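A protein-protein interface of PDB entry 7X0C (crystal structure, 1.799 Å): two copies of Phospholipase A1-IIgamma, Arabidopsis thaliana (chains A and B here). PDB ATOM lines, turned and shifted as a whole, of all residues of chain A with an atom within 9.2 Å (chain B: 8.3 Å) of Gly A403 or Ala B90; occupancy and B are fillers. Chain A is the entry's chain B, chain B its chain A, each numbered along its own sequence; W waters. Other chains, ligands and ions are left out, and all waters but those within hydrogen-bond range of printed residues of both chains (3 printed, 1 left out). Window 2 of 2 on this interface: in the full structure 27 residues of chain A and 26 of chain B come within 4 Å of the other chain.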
ATOM      1  N   ALA A 398      27.835 -23.156  28.547  1.00  0.00           N
ATOM      2  CA  ALA A 398      29.075 -22.440  28.805  1.00  0.00           C
ATOM      3  C   ALA A 398      29.237 -21.289  27.820  1.00  0.00           C
ATOM      4  O   ALA A 398      29.011 -21.435  26.613  1.00  0.00           O
ATOM      5  CB  ALA A 398      30.304 -23.367  28.703  1.00  0.00           C
ATOM      6  N   GLN A 399      29.655 -20.154  28.346  1.00  0.00           N
ATOM      7  CA  GLN A 399      30.002 -19.024  27.493  1.00  0.00           C
ATOM      8  C   GLN A 399      31.290 -19.309  26.718  1.00  0.00           C
ATOM      9  O   GLN A 399      32.309 -19.694  27.303  1.00  0.00           O
ATOM     10  CB  GLN A 399      30.145 -17.782  28.355  1.00  0.00           C
ATOM     11  CG  GLN A 399      30.294 -16.479  27.568  1.00  0.00           C
ATOM     12  CD  GLN A 399      30.392 -15.305  28.540  1.00  0.00           C
ATOM     13  OE1 GLN A 399      31.064 -15.404  29.573  1.00  0.00           O
ATOM     14  NE2 GLN A 399      29.719 -14.203  28.218  1.00  0.00           N
ATOM     15  N   GLN A 400      31.237 -19.115  25.402  1.00  0.00           N
ATOM     16  CA  GLN A 400      32.362 -19.323  24.493  1.00  0.00           C
ATOM     17  C   GLN A 400      33.110 -18.001  24.283  1.00  0.00           C
ATOM     18  O   GLN A 400      32.615 -16.924  24.616  1.00  0.00           O
ATOM     19  CB  GLN A 400      31.855 -19.892  23.153  1.00  0.00           C
ATOM     20  CG  GLN A 400      31.038 -21.170  23.308  1.00  0.00           C
ATOM     21  CD  GLN A 400      31.849 -22.235  24.023  1.00  0.00           C
ATOM     22  OE1 GLN A 400      32.933 -22.608  23.565  1.00  0.00           O
ATOM     23  NE2 GLN A 400      31.353 -22.709  25.172  1.00  0.00           N
ATOM     24  N   ASP A 401      34.317 -18.083  23.712  1.00  0.00           N
ATOM     25  CA  ASP A 401      35.157 -16.887  23.619  1.00  0.00           C
ATOM     26  C   ASP A 401      34.576 -15.815  22.719  1.00  0.00           C
ATOM     27  O   ASP A 401      34.995 -14.662  22.804  1.00  0.00           O
ATOM     28  CB  ASP A 401      36.550 -17.249  23.114  1.00  0.00           C
ATOM     29  CG  ASP A 401      37.385 -17.864  24.182  1.00  0.00           C
ATOM     30  OD1 ASP A 401      37.087 -17.618  25.373  1.00  0.00           O
ATOM     31  OD2 ASP A 401      38.321 -18.603  23.837  1.00  0.00           O
ATOM     32  N   ASP A 402      33.624 -16.153  21.859  1.00  0.00           N
ATOM     33  CA  ASP A 402      32.978 -15.162  21.015  1.00  0.00           C
ATOM     34  C   ASP A 402      31.667 -14.651  21.592  1.00  0.00           C
ATOM     35  O   ASP A 402      30.928 -13.966  20.878  1.00  0.00           O
ATOM     36  CB  ASP A 402      32.730 -15.737  19.616  1.00  0.00           C
ATOM     37  CG  ASP A 402      31.802 -16.949  19.633  1.00  0.00           C
ATOM     38  OD1 ASP A 402      31.390 -17.408  20.726  1.00  0.00           O
ATOM     39  OD2 ASP A 402      31.504 -17.474  18.538  1.00  0.00           O
ATOM     40  N   GLY A 403      31.361 -14.969  22.857  1.00  0.00           N
ATOM     41  CA  GLY A 403      30.121 -14.549  23.487  1.00  0.00           C
ATOM     42  C   GLY A 403      28.937 -15.471  23.259  1.00  0.00           C
ATOM     43  O   GLY A 403      27.880 -15.258  23.865  1.00  0.00           O
ATOM     44  N   SER A 404      29.073 -16.487  22.412  1.00  0.00           N
ATOM     45  CA  SER A 404      27.984 -17.434  22.241  1.00  0.00           C
ATOM     46  C   SER A 404      27.899 -18.321  23.487  1.00  0.00           C
ATOM     47  O   SER A 404      28.817 -18.365  24.312  1.00  0.00           O
ATOM     48  CB  SER A 404      28.180 -18.271  20.966  1.00  0.00           C
ATOM     49  OG  SER A 404      29.347 -19.059  21.061  1.00  0.00           O
ATOM     50  N   TRP A 405      26.766 -19.003  23.631  1.00  0.00           N
ATOM     51  CA  TRP A 405      26.518 -19.886  24.765  1.00  0.00           C
ATOM     52  C   TRP A 405      26.115 -21.234  24.191  1.00  0.00           C
ATOM     53  O   TRP A 405      25.142 -21.310  23.432  1.00  0.00           O
ATOM     54  CB  TRP A 405      25.405 -19.330  25.653  1.00  0.00           C
ATOM     55  CG  TRP A 405      25.882 -18.368  26.698  1.00  0.00           C
ATOM     56  CD1 TRP A 405      26.101 -17.016  26.559  1.00  0.00           C
ATOM     57  CD2 TRP A 405      26.191 -18.689  28.063  1.00  0.00           C
ATOM     58  NE1 TRP A 405      26.532 -16.490  27.762  1.00  0.00           N
ATOM     59  CE2 TRP A 405      26.582 -17.488  28.700  1.00  0.00           C
ATOM     60  CE3 TRP A 405      26.177 -19.874  28.802  1.00  0.00           C
ATOM     61  CZ2 TRP A 405      26.961 -17.434  30.049  1.00  0.00           C
ATOM     62  CZ3 TRP A 405      26.536 -19.812  30.170  1.00  0.00           C
ATOM     63  CH2 TRP A 405      26.927 -18.600  30.767  1.00  0.00           C
ATOM     64  N   GLU A 406      26.886 -22.279  24.522  1.00  0.00           N
ATOM     65  CA  GLU A 406      26.757 -23.595  23.902  1.00  0.00           C
ATOM     66  C   GLU A 406      26.706 -24.663  24.987  1.00  0.00           C
ATOM     67  O   GLU A 406      27.265 -24.492  26.066  1.00  0.00           O
ATOM     68  CB  GLU A 406      27.933 -23.878  22.954  1.00  0.00           C
ATOM     69  CG  GLU A 406      27.966 -22.940  21.703  1.00  0.00           C
ATOM     70  CD  GLU A 406      26.598 -22.727  21.013  1.00  0.00           C
ATOM     71  OE1 GLU A 406      26.308 -21.577  20.558  1.00  0.00           O
ATOM     72  OE2 GLU A 406      25.810 -23.709  20.909  1.00  0.00           O
ATOM     73  N   ILE B  15      32.756   0.621  17.928  1.00  0.00           N
ATOM     74  CA  ILE B  15      33.481   1.043  19.122  1.00  0.00           C
ATOM     75  C   ILE B  15      34.429   2.204  18.803  1.00  0.00           C
ATOM     76  O   ILE B  15      34.467   3.208  19.513  1.00  0.00           O
ATOM     77  CB  ILE B  15      34.230  -0.125  19.749  1.00  0.00           C
ATOM     78  CG1 ILE B  15      33.228  -1.094  20.384  1.00  0.00           C
ATOM     79  CG2 ILE B  15      35.195   0.377  20.784  1.00  0.00           C
ATOM     80  CD1 ILE B  15      33.871  -2.248  21.119  1.00  0.00           C
ATOM     81  N   GLU B  53      20.993  -6.459  31.299  1.00  0.00           N
ATOM     82  CA  GLU B  53      21.938  -7.467  31.765  1.00  0.00           C
ATOM     83  C   GLU B  53      22.401  -7.186  33.190  1.00  0.00           C
ATOM     84  O   GLU B  53      22.709  -8.123  33.937  1.00  0.00           O
ATOM     85  CB  GLU B  53      23.171  -7.526  30.859  1.00  0.00           C
ATOM     86  CG  GLU B  53      22.930  -8.216  29.560  1.00  0.00           C
ATOM     87  CD  GLU B  53      24.199  -8.215  28.683  1.00  0.00           C
ATOM     88  OE1 GLU B  53      24.974  -7.208  28.685  1.00  0.00           O
ATOM     89  OE2 GLU B  53      24.410  -9.213  27.981  1.00  0.00           O
ATOM     90  N   GLY B  86      29.243 -13.826  33.926  1.00  0.00           N
ATOM     91  CA  GLY B  86      29.225 -13.960  32.482  1.00  0.00           C
ATOM     92  C   GLY B  86      29.139 -12.667  31.710  1.00  0.00           C
ATOM     93  O   GLY B  86      28.740 -12.686  30.536  1.00  0.00           O
ATOM     94  N   LEU B  87      29.490 -11.541  32.327  1.00  0.00           N
ATOM     95  CA  LEU B  87      29.387 -10.233  31.682  1.00  0.00           C
ATOM     96  C   LEU B  87      30.764  -9.605  31.507  1.00  0.00           C
ATOM     97  O   LEU B  87      30.943  -8.395  31.662  1.00  0.00           O
ATOM     98  CB  LEU B  87      28.445  -9.299  32.454  1.00  0.00           C
ATOM     99  CG  LEU B  87      26.978  -9.746  32.548  1.00  0.00           C
ATOM    100  CD1 LEU B  87      26.113  -8.761  33.425  1.00  0.00           C
ATOM    101  CD2 LEU B  87      26.354  -9.878  31.134  1.00  0.00           C
ATOM    102  N   GLU B  88      31.751 -10.411  31.107  1.00  0.00           N
ATOM    103  CA  GLU B  88      33.049  -9.873  30.696  1.00  0.00           C
ATOM    104  C   GLU B  88      33.387 -10.252  29.261  1.00  0.00           C
ATOM    105  O   GLU B  88      33.606  -9.356  28.435  1.00  0.00           O
ATOM    106  CB  GLU B  88      34.140 -10.358  31.657  1.00  0.00           C
ATOM    107  CG  GLU B  88      35.531  -9.794  31.298  1.00  0.00           C
ATOM    108  CD  GLU B  88      36.569 -10.199  32.335  1.00  0.00           C
ATOM    109  OE1 GLU B  88      37.052 -11.350  32.292  1.00  0.00           O
ATOM    110  OE2 GLU B  88      36.854  -9.375  33.219  1.00  0.00           O
ATOM    111  N   ILE B  89      33.411 -11.553  28.943  1.00  0.00           N
ATOM    112  CA  ILE B  89      33.596 -12.003  27.570  1.00  0.00           C
ATOM    113  C   ILE B  89      32.552 -11.348  26.684  1.00  0.00           C
ATOM    114  O   ILE B  89      31.351 -11.378  26.991  1.00  0.00           O
ATOM    115  CB  ILE B  89      33.500 -13.537  27.495  1.00  0.00           C
ATOM    116  CG1 ILE B  89      34.607 -14.189  28.306  1.00  0.00           C
ATOM    117  CG2 ILE B  89      33.500 -13.998  26.039  1.00  0.00           C
ATOM    118  CD1 ILE B  89      34.367 -15.661  28.464  1.00  0.00           C
ATOM    119  N   ALA B  90      33.012 -10.719  25.597  1.00  0.00           N
ATOM    120  CA  ALA B  90      32.147 -10.066  24.606  1.00  0.00           C
ATOM    121  C   ALA B  90      31.242  -8.989  25.221  1.00  0.00           C
ATOM    122  O   ALA B  90      30.169  -8.675  24.688  1.00  0.00           O
ATOM    123  CB  ALA B  90      31.299 -11.087  23.832  1.00  0.00           C
ATOM    124  N   HIS B  91      31.682  -8.379  26.325  1.00  0.00           N
ATOM    125  CA  HIS B  91      30.986  -7.257  26.957  1.00  0.00           C
ATOM    126  C   HIS B  91      31.969  -6.111  27.167  1.00  0.00           C
ATOM    127  O   HIS B  91      32.282  -5.740  28.310  1.00  0.00           O
ATOM    128  CB  HIS B  91      30.355  -7.700  28.282  1.00  0.00           C
ATOM    129  CG  HIS B  91      29.150  -8.571  28.083  1.00  0.00           C
ATOM    130  ND1 HIS B  91      29.241  -9.895  27.718  1.00  0.00           N
ATOM    131  CD2 HIS B  91      27.829  -8.280  28.126  1.00  0.00           C
ATOM    132  CE1 HIS B  91      28.025 -10.387  27.547  1.00  0.00           C
ATOM    133  NE2 HIS B  91      27.150  -9.424  27.797  1.00  0.00           N
ATOM    134  N   PRO B  92      32.491  -5.544  26.075  1.00  0.00           N
ATOM    135  CA  PRO B  92      33.482  -4.457  26.190  1.00  0.00           C
ATOM    136  C   PRO B  92      32.987  -3.249  26.951  1.00  0.00           C
ATOM    137  O   PRO B  92      33.809  -2.506  27.499  1.00  0.00           O
ATOM    138  CB  PRO B  92      33.769  -4.096  24.724  1.00  0.00           C
ATOM    139  CG  PRO B  92      32.552  -4.526  23.979  1.00  0.00           C
ATOM    140  CD  PRO B  92      32.164  -5.825  24.664  1.00  0.00           C
ATOM    141  N   TYR B  93      31.674  -3.016  27.003  1.00  0.00           N
ATOM    142  CA  TYR B  93      31.147  -1.844  27.692  1.00  0.00           C
ATOM    143  C   TYR B  93      30.798  -2.097  29.151  1.00  0.00           C
ATOM    144  O   TYR B  93      30.422  -1.148  29.836  1.00  0.00           O
ATOM    145  CB  TYR B  93      29.890  -1.314  26.987  1.00  0.00           C
ATOM    146  CG  TYR B  93      30.147  -0.750  25.612  1.00  0.00           C
ATOM    147  CD1 TYR B  93      30.556   0.583  25.430  1.00  0.00           C
ATOM    148  CD2 TYR B  93      30.016  -1.560  24.485  1.00  0.00           C
ATOM    149  CE1 TYR B  93      30.802   1.084  24.137  1.00  0.00           C
ATOM    150  CE2 TYR B  93      30.266  -1.064  23.211  1.00  0.00           C
ATOM    151  CZ  TYR B  93      30.660   0.243  23.048  1.00  0.00           C
ATOM    152  OH  TYR B  93      30.897   0.688  21.768  1.00  0.00           O
ATOM    153  N   THR B  94      30.888  -3.329  29.650  1.00  0.00           N
ATOM    154  CA  THR B  94      30.496  -3.590  31.041  1.00  0.00           C
ATOM    155  C   THR B  94      31.724  -3.470  31.952  1.00  0.00           C
ATOM    156  O   THR B  94      32.085  -4.360  32.703  1.00  0.00           O
ATOM    157  CB  THR B  94      29.806  -4.952  31.164  1.00  0.00           C
ATOM    158  OG1 THR B  94      28.808  -5.046  30.135  1.00  0.00           O
ATOM    159  CG2 THR B  94      29.100  -5.063  32.528  1.00  0.00           C
ATOM    160  N   LYS B  95      32.353  -2.305  31.867  1.00  0.00           N
ATOM    161  CA  LYS B  95      33.569  -2.014  32.628  1.00  0.00           C
ATOM    162  C   LYS B  95      33.189  -1.278  33.908  1.00  0.00           C
ATOM    163  O   LYS B  95      33.452  -0.086  34.071  1.00  0.00           O
ATOM    164  CB  LYS B  95      34.540  -1.188  31.791  1.00  0.00           C
ATOM    165  CG  LYS B  95      35.037  -1.879  30.496  1.00  0.00           C
ATOM    166  CD  LYS B  95      35.651  -3.234  30.782  1.00  0.00           C
ATOM    167  CE  LYS B  95      36.333  -3.822  29.503  1.00  0.00           C
ATOM    168  NZ  LYS B  95      36.873  -5.206  29.740  1.00  0.00           N
ATOM    169  N   GLU B 366      24.006 -10.027  18.281  1.00  0.00           N
ATOM    170  CA  GLU B 366      24.427 -11.431  18.392  1.00  0.00           C
ATOM    171  C   GLU B 366      24.160 -11.997  19.792  1.00  0.00           C
ATOM    172  O   GLU B 366      25.064 -12.449  20.490  1.00  0.00           O
ATOM    173  CB  GLU B 366      25.906 -11.575  18.061  1.00  0.00           C
ATOM    174  CG  GLU B 366      26.271 -11.396  16.607  1.00  0.00           C
ATOM    175  CD  GLU B 366      27.783 -11.502  16.383  1.00  0.00           C
ATOM    176  OE1 GLU B 366      28.533 -11.718  17.371  1.00  0.00           O
ATOM    177  OE2 GLU B 366      28.222 -11.365  15.221  1.00  0.00           O
ATOM    178  N   ARG B 367      22.908 -11.962  20.214  1.00  0.00           N
ATOM    179  CA  ARG B 367      22.587 -12.370  21.592  1.00  0.00           C
ATOM    180  C   ARG B 367      22.225 -13.858  21.627  1.00  0.00           C
ATOM    181  O   ARG B 367      21.257 -14.281  20.989  1.00  0.00           O
ATOM    182  CB  ARG B 367      21.440 -11.524  22.150  1.00  0.00           C
ATOM    183  CG  ARG B 367      21.152 -11.838  23.633  1.00  0.00           C
ATOM    184  CD  ARG B 367      20.314 -10.742  24.328  1.00  0.00           C
ATOM    185  NE  ARG B 367      20.264 -11.015  25.762  1.00  0.00           N
ATOM    186  CZ  ARG B 367      21.253 -10.723  26.624  1.00  0.00           C
ATOM    187  NH1 ARG B 367      22.351 -10.118  26.200  1.00  0.00           N
ATOM    188  NH2 ARG B 367      21.147 -11.086  27.922  1.00  0.00           N
ATOM    189  N   ALA B 368      22.974 -14.644  22.404  1.00  0.00           N
ATOM    190  CA  ALA B 368      22.780 -16.091  22.419  1.00  0.00           C
ATOM    191  C   ALA B 368      21.368 -16.444  22.870  1.00  0.00           C
ATOM    192  O   ALA B 368      20.939 -16.073  23.976  1.00  0.00           O
ATOM    193  CB  ALA B 368      23.823 -16.750  23.339  1.00  0.00           C
ATOM    194  N   ILE B 369      20.637 -17.178  22.023  1.00  0.00           N
ATOM    195  CA  ILE B 369      19.264 -17.493  22.399  1.00  0.00           C
ATOM    196  C   ILE B 369      19.241 -18.378  23.632  1.00  0.00           C
ATOM    197  O   ILE B 369      18.260 -18.365  24.384  1.00  0.00           O
ATOM    198  CB  ILE B 369      18.488 -18.152  21.244  1.00  0.00           C
ATOM    199  CG1 ILE B 369      19.110 -19.490  20.853  1.00  0.00           C
ATOM    200  CG2 ILE B 369      18.449 -17.195  20.040  1.00  0.00           C
ATOM    201  CD1 ILE B 369      18.273 -20.265  19.818  1.00  0.00           C
ATOM    202  N   LEU B 371      20.386 -18.020  26.400  1.00  0.00           N
ATOM    203  CA  LEU B 371      20.249 -17.294  27.653  1.00  0.00           C
ATOM    204  C   LEU B 371      18.812 -17.291  28.154  1.00  0.00           C
ATOM    205  O   LEU B 371      18.579 -17.145  29.358  1.00  0.00           O
ATOM    206  CB  LEU B 371      20.731 -15.845  27.466  1.00  0.00           C
ATOM    207  CG  LEU B 371      22.227 -15.763  27.167  1.00  0.00           C
ATOM    208  CD1 LEU B 371      22.600 -14.353  26.645  1.00  0.00           C
ATOM    209  CD2 LEU B 371      22.980 -16.050  28.450  1.00  0.00           C
HETATM  210  O   HOH W   1      25.399 -13.675  23.706  1.00  0.00           O
HETATM  211  O   HOH W   2      22.566 -20.046  22.479  1.00  0.00           O
HETATM  212  O   HOH W   3      26.410 -13.815  29.411  1.00  0.00           O
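The backbone carbonyl oxygen of Gly B86 sits at hydrogen-bond distance from the side-chain amide nitrogen of Gln A399.
The side-chain amide nitrogen (NE2) of Gln A399 is in hydrogen-bond range of the backbone carbonyl oxygen (O) of Ile B89 (3.5 Å).
O of Ile B89 is in hydrogen-bond range of ND1 of His B91.
The backbone carbonyl oxygen (O) of Ala A398 lies within hydrogen-bond range of the side-chain amide nitrogen (NE2) of Gln A400 (3.0 Å).
Among the printed residues, pairs that only touch across the chains: Gln A400 with Ile B89 (3.4 Å), Asp A401 with Ile B89 (3.6 Å), Gly A403 with Ile B89 (3.96 Å), Gly A403 with Ala B90 (3.7 Å), Trp A405 with Ala B368 (3.7 Å) and Trp A405 with Leu B371 (3.6 Å).
No residue of chain B comes within 4 Å of Ser A404.
Printed residues of chain A within 4 Å of Leu B371: Trp A405.
Printed residues of chain B within 4 Å of Gln A400: Ile B89.
Of the printed residues of chain B, Asp A401 touches Ile B89.
Of the printed residues of chain A, Ala B368 touches Trp A405.
Glu B366 touches none of the printed residues of chain A.
Pro B92 touches none of the printed residues of chain A.
The nearest residue of chain B that does not touch Gly A403 is Ala B368 (4.4 Å).
Hydrophobic or aromatic side chains of chain B that line the printed part of chain A: Ile B89, Ala B90, Ala B368 and Leu B371.
Of the 9 printed residues of chain A, 5 touch a printed residue of chain B.
No position is printed for both chains.
Water W3 lies within hydrogen-bond range of O of Gly B86 (2.8 Å) and NE1 of Trp A405 (3.1 Å).
Water W1 lies within hydrogen-bond range of N of Ala B368, O of Gly A403 and O of Glu B366.
Water W2 bridges O of Trp A405 (3.0 Å) and N of Ile B369 (3.5 Å).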
